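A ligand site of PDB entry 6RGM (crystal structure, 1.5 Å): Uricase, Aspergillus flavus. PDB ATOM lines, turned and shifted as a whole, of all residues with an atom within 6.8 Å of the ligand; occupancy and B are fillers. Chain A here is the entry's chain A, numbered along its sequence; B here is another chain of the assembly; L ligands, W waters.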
ATOM      1  N   SER A 158      23.613 -12.535 -10.521  1.00  0.00           N
ATOM      2  CA  SER A 158      24.077 -11.158 -10.581  1.00  0.00           C
ATOM      3  C   SER A 158      24.601 -10.896 -11.973  1.00  0.00           C
ATOM      4  O   SER A 158      25.278 -11.780 -12.524  1.00  0.00           O
ATOM      5  CB  SER A 158      25.138 -10.875  -9.492  1.00  0.00           C
ATOM      6  OG  SER A 158      25.663  -9.564  -9.648  1.00  0.00           O
ATOM      7  N   GLN A 159      24.229  -9.731 -12.502  1.00  0.00           N
ATOM      8  CA  GLN A 159      24.598  -9.335 -13.850  1.00  0.00           C
ATOM      9  C   GLN A 159      25.129  -7.910 -13.830  1.00  0.00           C
ATOM     10  O   GLN A 159      24.767  -7.131 -12.927  1.00  0.00           O
ATOM     11  CB  GLN A 159      23.365  -9.441 -14.771  1.00  0.00           C
ATOM     12  CG  GLN A 159      22.712 -10.819 -14.687  1.00  0.00           C
ATOM     13  CD  GLN A 159      21.576 -10.906 -15.684  1.00  0.00           C
ATOM     14  OE1 GLN A 159      21.685 -10.410 -16.788  1.00  0.00           O
ATOM     15  NE2 GLN A 159      20.506 -11.547 -15.276  1.00  0.00           N
ATOM     16  N   PHE A 160      25.856  -7.514 -14.860  1.00  0.00           N
ATOM     17  CA  PHE A 160      26.206  -6.096 -15.019  1.00  0.00           C
ATOM     18  C   PHE A 160      26.571  -5.829 -16.457  1.00  0.00           C
ATOM     19  O   PHE A 160      27.658  -6.131 -16.937  1.00  0.00           O
ATOM     20  CB  PHE A 160      27.275  -5.618 -14.014  1.00  0.00           C
ATOM     21  CG  PHE A 160      27.397  -4.128 -13.982  1.00  0.00           C
ATOM     22  CD1 PHE A 160      26.334  -3.345 -13.593  1.00  0.00           C
ATOM     23  CD2 PHE A 160      28.522  -3.479 -14.488  1.00  0.00           C
ATOM     24  CE1 PHE A 160      26.423  -1.976 -13.625  1.00  0.00           C
ATOM     25  CE2 PHE A 160      28.635  -2.108 -14.488  1.00  0.00           C
ATOM     26  CZ  PHE A 160      27.564  -1.345 -14.045  1.00  0.00           C
ATOM     27  N   PHE A 163      26.083  -0.715 -19.353  1.00  0.00           N
ATOM     28  CA  PHE A 163      26.663   0.516 -18.786  1.00  0.00           C
ATOM     29  C   PHE A 163      27.366   1.325 -19.868  1.00  0.00           C
ATOM     30  O   PHE A 163      27.612   0.794 -20.977  1.00  0.00           O
ATOM     31  CB  PHE A 163      27.635   0.206 -17.645  1.00  0.00           C
ATOM     32  CG  PHE A 163      28.644  -0.875 -17.958  1.00  0.00           C
ATOM     33  CD1 PHE A 163      29.845  -0.521 -18.529  1.00  0.00           C
ATOM     34  CD2 PHE A 163      28.382  -2.222 -17.691  1.00  0.00           C
ATOM     35  CE1 PHE A 163      30.805  -1.489 -18.804  1.00  0.00           C
ATOM     36  CE2 PHE A 163      29.339  -3.187 -17.998  1.00  0.00           C
ATOM     37  CZ  PHE A 163      30.523  -2.813 -18.594  1.00  0.00           C
ATOM     38  N   LEU A 171      35.917  -2.660 -18.916  1.00  0.00           N
ATOM     39  CA  LEU A 171      35.140  -3.723 -18.256  1.00  0.00           C
ATOM     40  C   LEU A 171      34.265  -4.478 -19.267  1.00  0.00           C
ATOM     41  O   LEU A 171      33.485  -3.841 -20.029  1.00  0.00           O
ATOM     42  CB  LEU A 171      34.255  -3.064 -17.198  1.00  0.00           C
ATOM     43  CG  LEU A 171      33.379  -4.025 -16.381  1.00  0.00           C
ATOM     44  CD1 LEU A 171      34.243  -4.973 -15.568  1.00  0.00           C
ATOM     45  CD2 LEU A 171      32.460  -3.251 -15.488  1.00  0.00           C
ATOM     46  N   ARG A 177      27.782 -13.166 -12.799  1.00  0.00           N
ATOM     47  CA  ARG A 177      28.975 -12.855 -11.978  1.00  0.00           C
ATOM     48  C   ARG A 177      28.646 -13.182 -10.526  1.00  0.00           C
ATOM     49  O   ARG A 177      27.483 -13.352 -10.126  1.00  0.00           O
ATOM     50  CB  ARG A 177      29.392 -11.407 -12.126  1.00  0.00           C
ATOM     51  CG  ARG A 177      28.396 -10.393 -11.545  1.00  0.00           C
ATOM     52  CD  ARG A 177      28.822  -8.939 -11.643  1.00  0.00           C
ATOM     53  NE  ARG A 177      27.863  -8.095 -10.969  1.00  0.00           N
ATOM     54  CZ  ARG A 177      28.031  -6.781 -10.740  1.00  0.00           C
ATOM     55  NH1 ARG A 177      29.076  -6.128 -11.234  1.00  0.00           N
ATOM     56  NH2 ARG A 177      27.109  -6.127 -10.061  1.00  0.00           N
ATOM     57  N   LEU A 179      28.347 -11.697  -6.743  1.00  0.00           N
ATOM     58  CA  LEU A 179      28.114 -10.431  -6.033  1.00  0.00           C
ATOM     59  C   LEU A 179      28.328 -10.651  -4.540  1.00  0.00           C
ATOM     60  O   LEU A 179      27.690 -11.537  -3.938  1.00  0.00           O
ATOM     61  CB  LEU A 179      26.707  -9.911  -6.334  1.00  0.00           C
ATOM     62  CG  LEU A 179      26.344  -8.625  -5.599  1.00  0.00           C
ATOM     63  CD1 LEU A 179      27.298  -7.498  -5.989  1.00  0.00           C
ATOM     64  CD2 LEU A 179      24.877  -8.256  -5.890  1.00  0.00           C
ATOM     65  N   SER A 225      20.019  -9.808  -9.995  1.00  0.00           N
ATOM     66  CA  SER A 225      20.434  -8.407  -9.850  1.00  0.00           C
ATOM     67  C   SER A 225      20.981  -7.813 -11.134  1.00  0.00           C
ATOM     68  O   SER A 225      21.912  -8.360 -11.728  1.00  0.00           O
ATOM     69  CB  SER A 225      21.490  -8.358  -8.742  1.00  0.00           C
ATOM     70  OG  SER A 225      22.039  -7.049  -8.660  1.00  0.00           O
ATOM     71  N   ALA A 226      20.471  -6.644 -11.513  1.00  0.00           N
ATOM     72  CA  ALA A 226      20.895  -5.873 -12.685  1.00  0.00           C
ATOM     73  C   ALA A 226      22.147  -5.052 -12.374  1.00  0.00           C
ATOM     74  O   ALA A 226      22.851  -4.604 -13.282  1.00  0.00           O
ATOM     75  CB  ALA A 226      19.779  -4.990 -13.153  1.00  0.00           C
ATOM     76  N   SER A 227      22.326  -4.771 -11.071  1.00  0.00           N
ATOM     77  CA  SER A 227      23.382  -3.885 -10.544  1.00  0.00           C
ATOM     78  C   SER A 227      23.200  -3.848  -9.049  1.00  0.00           C
ATOM     79  O   SER A 227      22.132  -4.147  -8.526  1.00  0.00           O
ATOM     80  CB  SER A 227      23.375  -2.489 -11.109  1.00  0.00           C
ATOM     81  OG  SER A 227      22.192  -1.825 -10.650  1.00  0.00           O
ATOM     82  N   VAL A 228      24.263  -3.459  -8.335  1.00  0.00           N
ATOM     83  CA  VAL A 228      24.109  -3.154  -6.904  1.00  0.00           C
ATOM     84  C   VAL A 228      23.036  -2.064  -6.721  1.00  0.00           C
ATOM     85  O   VAL A 228      22.199  -2.216  -5.825  1.00  0.00           O
ATOM     86  CB  VAL A 228      25.457  -2.745  -6.299  1.00  0.00           C
ATOM     87  CG1 VAL A 228      25.302  -2.310  -4.870  1.00  0.00           C
ATOM     88  CG2 VAL A 228      26.456  -3.897  -6.387  1.00  0.00           C
ATOM     89  N   GLN A 229      23.096  -1.024  -7.525  1.00  0.00           N
ATOM     90  CA  GLN A 229      22.145   0.113  -7.491  1.00  0.00           C
ATOM     91  C   GLN A 229      20.721  -0.442  -7.487  1.00  0.00           C
ATOM     92  O   GLN A 229      19.900  -0.022  -6.657  1.00  0.00           O
ATOM     93  CB  GLN A 229      22.388   1.047  -8.688  1.00  0.00           C
ATOM     94  CG  GLN A 229      23.679   1.850  -8.685  1.00  0.00           C
ATOM     95  CD  GLN A 229      24.923   1.185  -9.241  1.00  0.00           C
ATOM     96  OE1 GLN A 229      25.060  -0.035  -9.234  1.00  0.00           O
ATOM     97  NE2 GLN A 229      25.862   2.021  -9.705  1.00  0.00           N
ATOM     98  N   ASN A 255      31.154  -3.143  -3.525  1.00  0.00           N
ATOM     99  CA  ASN A 255      31.115  -4.259  -4.488  1.00  0.00           C
ATOM    100  C   ASN A 255      32.475  -4.935  -4.349  1.00  0.00           C
ATOM    101  O   ASN A 255      33.461  -4.367  -4.783  1.00  0.00           O
ATOM    102  CB  ASN A 255      30.816  -3.748  -5.897  1.00  0.00           C
ATOM    103  CG  ASN A 255      30.479  -4.858  -6.869  1.00  0.00           C
ATOM    104  OD1 ASN A 255      30.460  -6.005  -6.482  1.00  0.00           O
ATOM    105  ND2 ASN A 255      30.240  -4.496  -8.125  1.00  0.00           N
ATOM    106  N   HIS A 257      34.881  -7.298  -5.302  1.00  0.00           N
ATOM    107  CA  HIS A 257      35.048  -7.966  -6.609  1.00  0.00           C
ATOM    108  C   HIS A 257      35.714  -9.330  -6.467  1.00  0.00           C
ATOM    109  O   HIS A 257      36.704  -9.459  -5.711  1.00  0.00           O
ATOM    110  CB  HIS A 257      35.844  -7.088  -7.551  1.00  0.00           C
ATOM    111  CG  HIS A 257      35.261  -5.719  -7.727  1.00  0.00           C
ATOM    112  ND1 HIS A 257      34.020  -5.473  -8.301  1.00  0.00           N
ATOM    113  CD2 HIS A 257      35.773  -4.511  -7.407  1.00  0.00           C
ATOM    114  CE1 HIS A 257      33.808  -4.157  -8.261  1.00  0.00           C
ATOM    115  NE2 HIS A 257      34.863  -3.557  -7.726  1.00  0.00           N
ATOM    116  N   GLY A 287      34.218  -1.202  -5.753  1.00  0.00           N
ATOM    117  CA  GLY A 287      33.065  -0.324  -5.959  1.00  0.00           C
ATOM    118  C   GLY A 287      32.456   0.097  -4.641  1.00  0.00           C
ATOM    119  O   GLY A 287      32.486  -0.660  -3.673  1.00  0.00           O
ATOM    120  N   ILE A 289      28.767   1.960  -3.548  1.00  0.00           N
ATOM    121  CA  ILE A 289      27.445   2.342  -4.102  1.00  0.00           C
ATOM    122  C   ILE A 289      26.586   2.812  -2.938  1.00  0.00           C
ATOM    123  O   ILE A 289      26.435   2.057  -1.956  1.00  0.00           O
ATOM    124  CB  ILE A 289      26.831   1.143  -4.850  1.00  0.00           C
ATOM    125  CG1 ILE A 289      27.815   0.338  -5.712  1.00  0.00           C
ATOM    126  CG2 ILE A 289      25.640   1.634  -5.656  1.00  0.00           C
ATOM    127  CD1 ILE A 289      28.507   1.096  -6.806  1.00  0.00           C
ATOM    128  N   TYR B   9      28.029   7.059  -6.270  1.00  0.00           N
ATOM    129  CA  TYR B   9      28.642   5.728  -6.465  1.00  0.00           C
ATOM    130  C   TYR B   9      29.997   5.930  -7.149  1.00  0.00           C
ATOM    131  O   TYR B   9      30.219   6.921  -7.776  1.00  0.00           O
ATOM    132  CB  TYR B   9      27.687   4.827  -7.275  1.00  0.00           C
ATOM    133  CG  TYR B   9      27.903   5.087  -8.736  1.00  0.00           C
ATOM    134  CD1 TYR B   9      27.443   6.249  -9.303  1.00  0.00           C
ATOM    135  CD2 TYR B   9      28.723   4.270  -9.478  1.00  0.00           C
ATOM    136  CE1 TYR B   9      27.750   6.579 -10.615  1.00  0.00           C
ATOM    137  CE2 TYR B   9      29.042   4.587 -10.776  1.00  0.00           C
ATOM    138  CZ  TYR B   9      28.544   5.730 -11.354  1.00  0.00           C
ATOM    139  OH  TYR B   9      28.861   6.067 -12.615  1.00  0.00           O
ATOM    140  N   GLY B  10      30.879   4.973  -6.965  1.00  0.00           N
ATOM    141  CA  GLY B  10      32.182   5.049  -7.621  1.00  0.00           C
ATOM    142  C   GLY B  10      33.132   3.990  -7.118  1.00  0.00           C
ATOM    143  O   GLY B  10      32.708   2.950  -6.776  1.00  0.00           O
ATOM    144  N   LYS B  11      34.409   4.326  -7.159  1.00  0.00           N
ATOM    145  CA  LYS B  11      35.459   3.362  -6.755  1.00  0.00           C
ATOM    146  C   LYS B  11      36.180   3.905  -5.518  1.00  0.00           C
ATOM    147  O   LYS B  11      36.643   5.043  -5.537  1.00  0.00           O
ATOM    148  CB  LYS B  11      36.456   3.091  -7.880  1.00  0.00           C
ATOM    149  CG  LYS B  11      37.247   1.816  -7.629  1.00  0.00           C
ATOM    150  CD  LYS B  11      36.438   0.554  -7.835  1.00  0.00           C
ATOM    151  CE  LYS B  11      36.633  -0.133  -9.146  1.00  0.00           C
ATOM    152  NZ  LYS B  11      35.572  -1.146  -9.427  1.00  0.00           N
ATOM    153  N   ASN B  52      21.297   0.877 -16.675  1.00  0.00           N
ATOM    154  CA  ASN B  52      22.775   1.018 -16.522  1.00  0.00           C
ATOM    155  C   ASN B  52      23.351   1.975 -17.539  1.00  0.00           C
ATOM    156  O   ASN B  52      24.514   2.369 -17.397  1.00  0.00           O
ATOM    157  CB  ASN B  52      23.464  -0.351 -16.530  1.00  0.00           C
ATOM    158  CG  ASN B  52      23.123  -1.175 -15.310  1.00  0.00           C
ATOM    159  OD1 ASN B  52      22.833  -0.575 -14.257  1.00  0.00           O
ATOM    160  ND2 ASN B  52      23.181  -2.494 -15.395  1.00  0.00           N
ATOM    161  N   ILE B  55      25.292   4.763 -16.043  1.00  0.00           N
ATOM    162  CA  ILE B  55      26.446   4.419 -15.154  1.00  0.00           C
ATOM    163  C   ILE B  55      27.747   4.474 -15.940  1.00  0.00           C
ATOM    164  O   ILE B  55      27.950   3.668 -16.863  1.00  0.00           O
ATOM    165  CB  ILE B  55      26.231   3.050 -14.492  1.00  0.00           C
ATOM    166  CG1 ILE B  55      24.985   2.995 -13.620  1.00  0.00           C
ATOM    167  CG2 ILE B  55      27.475   2.703 -13.645  1.00  0.00           C
ATOM    168  CD1 ILE B  55      24.750   1.597 -13.066  1.00  0.00           C
ATOM    169  N   VAL B  56      28.646   5.345 -15.496  1.00  0.00           N
ATOM    170  CA  VAL B  56      30.111   5.285 -15.799  1.00  0.00           C
ATOM    171  C   VAL B  56      30.624   4.188 -14.871  1.00  0.00           C
ATOM    172  O   VAL B  56      30.575   4.396 -13.648  1.00  0.00           O
ATOM    173  CB  VAL B  56      30.805   6.615 -15.524  1.00  0.00           C
ATOM    174  CG1 VAL B  56      32.309   6.541 -15.749  1.00  0.00           C
ATOM    175  CG2 VAL B  56      30.178   7.729 -16.384  1.00  0.00           C
ATOM    176  N   ALA B  57      31.005   3.034 -15.393  1.00  0.00           N
ATOM    177  CA  ALA B  57      31.313   1.872 -14.534  1.00  0.00           C
ATOM    178  C   ALA B  57      32.334   2.300 -13.474  1.00  0.00           C
ATOM    179  O   ALA B  57      33.284   3.016 -13.824  1.00  0.00           O
ATOM    180  CB  ALA B  57      31.855   0.725 -15.347  1.00  0.00           C
ATOM    181  N   THR B  58      32.243   1.740 -12.266  1.00  0.00           N
ATOM    182  CA  THR B  58      33.295   1.999 -11.245  1.00  0.00           C
ATOM    183  C   THR B  58      34.653   1.544 -11.796  1.00  0.00           C
ATOM    184  O   THR B  58      35.662   2.173 -11.474  1.00  0.00           O
ATOM    185  CB  THR B  58      32.931   1.388  -9.880  1.00  0.00           C
ATOM    186  OG1 THR B  58      33.049  -0.021  -9.944  1.00  0.00           O
ATOM    187  CG2 THR B  58      31.564   1.801  -9.415  1.00  0.00           C
ATOM    188  N   ASP B  59      34.714   0.444 -12.539  1.00  0.00           N
ATOM    189  CA  ASP B  59      35.989   0.010 -13.162  1.00  0.00           C
ATOM    190  C   ASP B  59      36.538   1.121 -14.055  1.00  0.00           C
ATOM    191  O   ASP B  59      37.736   1.280 -14.134  1.00  0.00           O
ATOM    192  CB  ASP B  59      35.749  -1.277 -13.952  1.00  0.00           C
ATOM    193  CG  ASP B  59      37.039  -1.882 -14.412  1.00  0.00           C
ATOM    194  OD1 ASP B  59      37.715  -2.529 -13.567  1.00  0.00           O
ATOM    195  OD2 ASP B  59      37.430  -1.652 -15.607  1.00  0.00           O
ATOM    196  N   SER B  60      35.684   1.786 -14.828  1.00  0.00           N
ATOM    197  CA  SER B  60      36.116   2.918 -15.675  1.00  0.00           C
ATOM    198  C   SER B  60      36.631   4.085 -14.838  1.00  0.00           C
ATOM    199  O   SER B  60      37.576   4.773 -15.235  1.00  0.00           O
ATOM    200  CB  SER B  60      34.990   3.371 -16.579  1.00  0.00           C
ATOM    201  OG  SER B  60      34.567   2.269 -17.347  1.00  0.00           O
HETATM  202  N1  LIG L   1      27.537  -1.285 -10.299  1.00  0.00           N
HETATM  203  C1  LIG L   1      27.615  -2.654 -10.282  1.00  0.00           C
HETATM  204  O1  LIG L   1      26.770  -3.364  -9.770  1.00  0.00           O
HETATM  205  N2  LIG L   1      28.769  -3.203 -10.764  1.00  0.00           N
HETATM  206  C2  LIG L   1      29.677  -2.413 -11.314  1.00  0.00           C
HETATM  207  C3  LIG L   1      29.539  -1.020 -11.412  1.00  0.00           C
HETATM  208  C4  LIG L   1      28.394  -0.384 -10.873  1.00  0.00           C
HETATM  209  O2  LIG L   1      28.140   0.826 -10.808  1.00  0.00           O
HETATM  210  N3  LIG L   1      30.664  -0.523 -12.004  1.00  0.00           N
HETATM  211  N4  LIG L   1      31.449  -1.527 -12.280  1.00  0.00           N
HETATM  212  N5  LIG L   1      30.872  -2.663 -11.884  1.00  0.00           N
HETATM  213  O   HOH W   1      32.211  -5.154 -11.834  1.00  0.00           O
HETATM  214  O   HOH W   2      31.168  -1.562  -8.469  1.00  0.00           O
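Residues that only touch the ligand: Phe 160, Leu 171, Ser 227, Tyr 9 of chain B, Ile 55 of chain B, Ala 57 of chain B and Asp 59 of chain B.
Hydrophobic or aromatic side chains within 4 Å of the ligand: Phe 160, Leu 171, Val 228, Tyr 9 of chain B, Ile 55 of chain B and Ala 57 of chain B.
The nearest printed residue that does not touch the ligand is Ile 289 (4.03 Å).
OG1 of Thr 58 of chain B sits at hydrogen-bond distance from N3 of the ligand.
NE2 of Gln 229 sits at hydrogen-bond distance from O2 of the ligand, 2.8 Å away.
NH2 of Arg 177 is in hydrogen-bond range of O1 of the ligand, 2.8 Å away.
N3 of the ligand lies within hydrogen-bond range of N of Thr 58 of chain B, 2.8 Å away.
N of Val 228 is in hydrogen-bond range of O1 of the ligand (2.9 Å).
ND2 of Asn 255 sits close to N2 of the ligand.
The backbone NH (N) of Asn 255 lies within hydrogen-bond range of the backbone carbonyl oxygen (O) of Gly 287 (2.8 Å).
The backbone carbonyl oxygen of Ser 227 lies within hydrogen-bond range of the side-chain hydroxyl of Ser 225 (2.9 Å).
N of Arg 177 lies within hydrogen-bond range of O of Ser 158 (2.9 Å).
The side-chain hydroxyl (OH) of Tyr 9 of chain B is in hydrogen-bond range of the backbone carbonyl oxygen (O) of Val 56 of chain B (2.6 Å).
N of Gln 229 lies close to OG of Ser 227 (3.4 Å).
O of Asn 255 sits at hydrogen-bond distance from NE2 of His 257 (3.4 Å).
NZ of Lys 11 of chain B sits at hydrogen-bond distance from OG1 of Thr 58 of chain B (2.8 Å).
Water W1 lies within hydrogen-bond range of N5 of the ligand (2.8 Å) and NH1 of Arg 177 (3.3 Å).
Water W2 bridges the side-chain hydroxyl of Thr 58 of chain B and the side-chain amide nitrogen of Asn 255.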
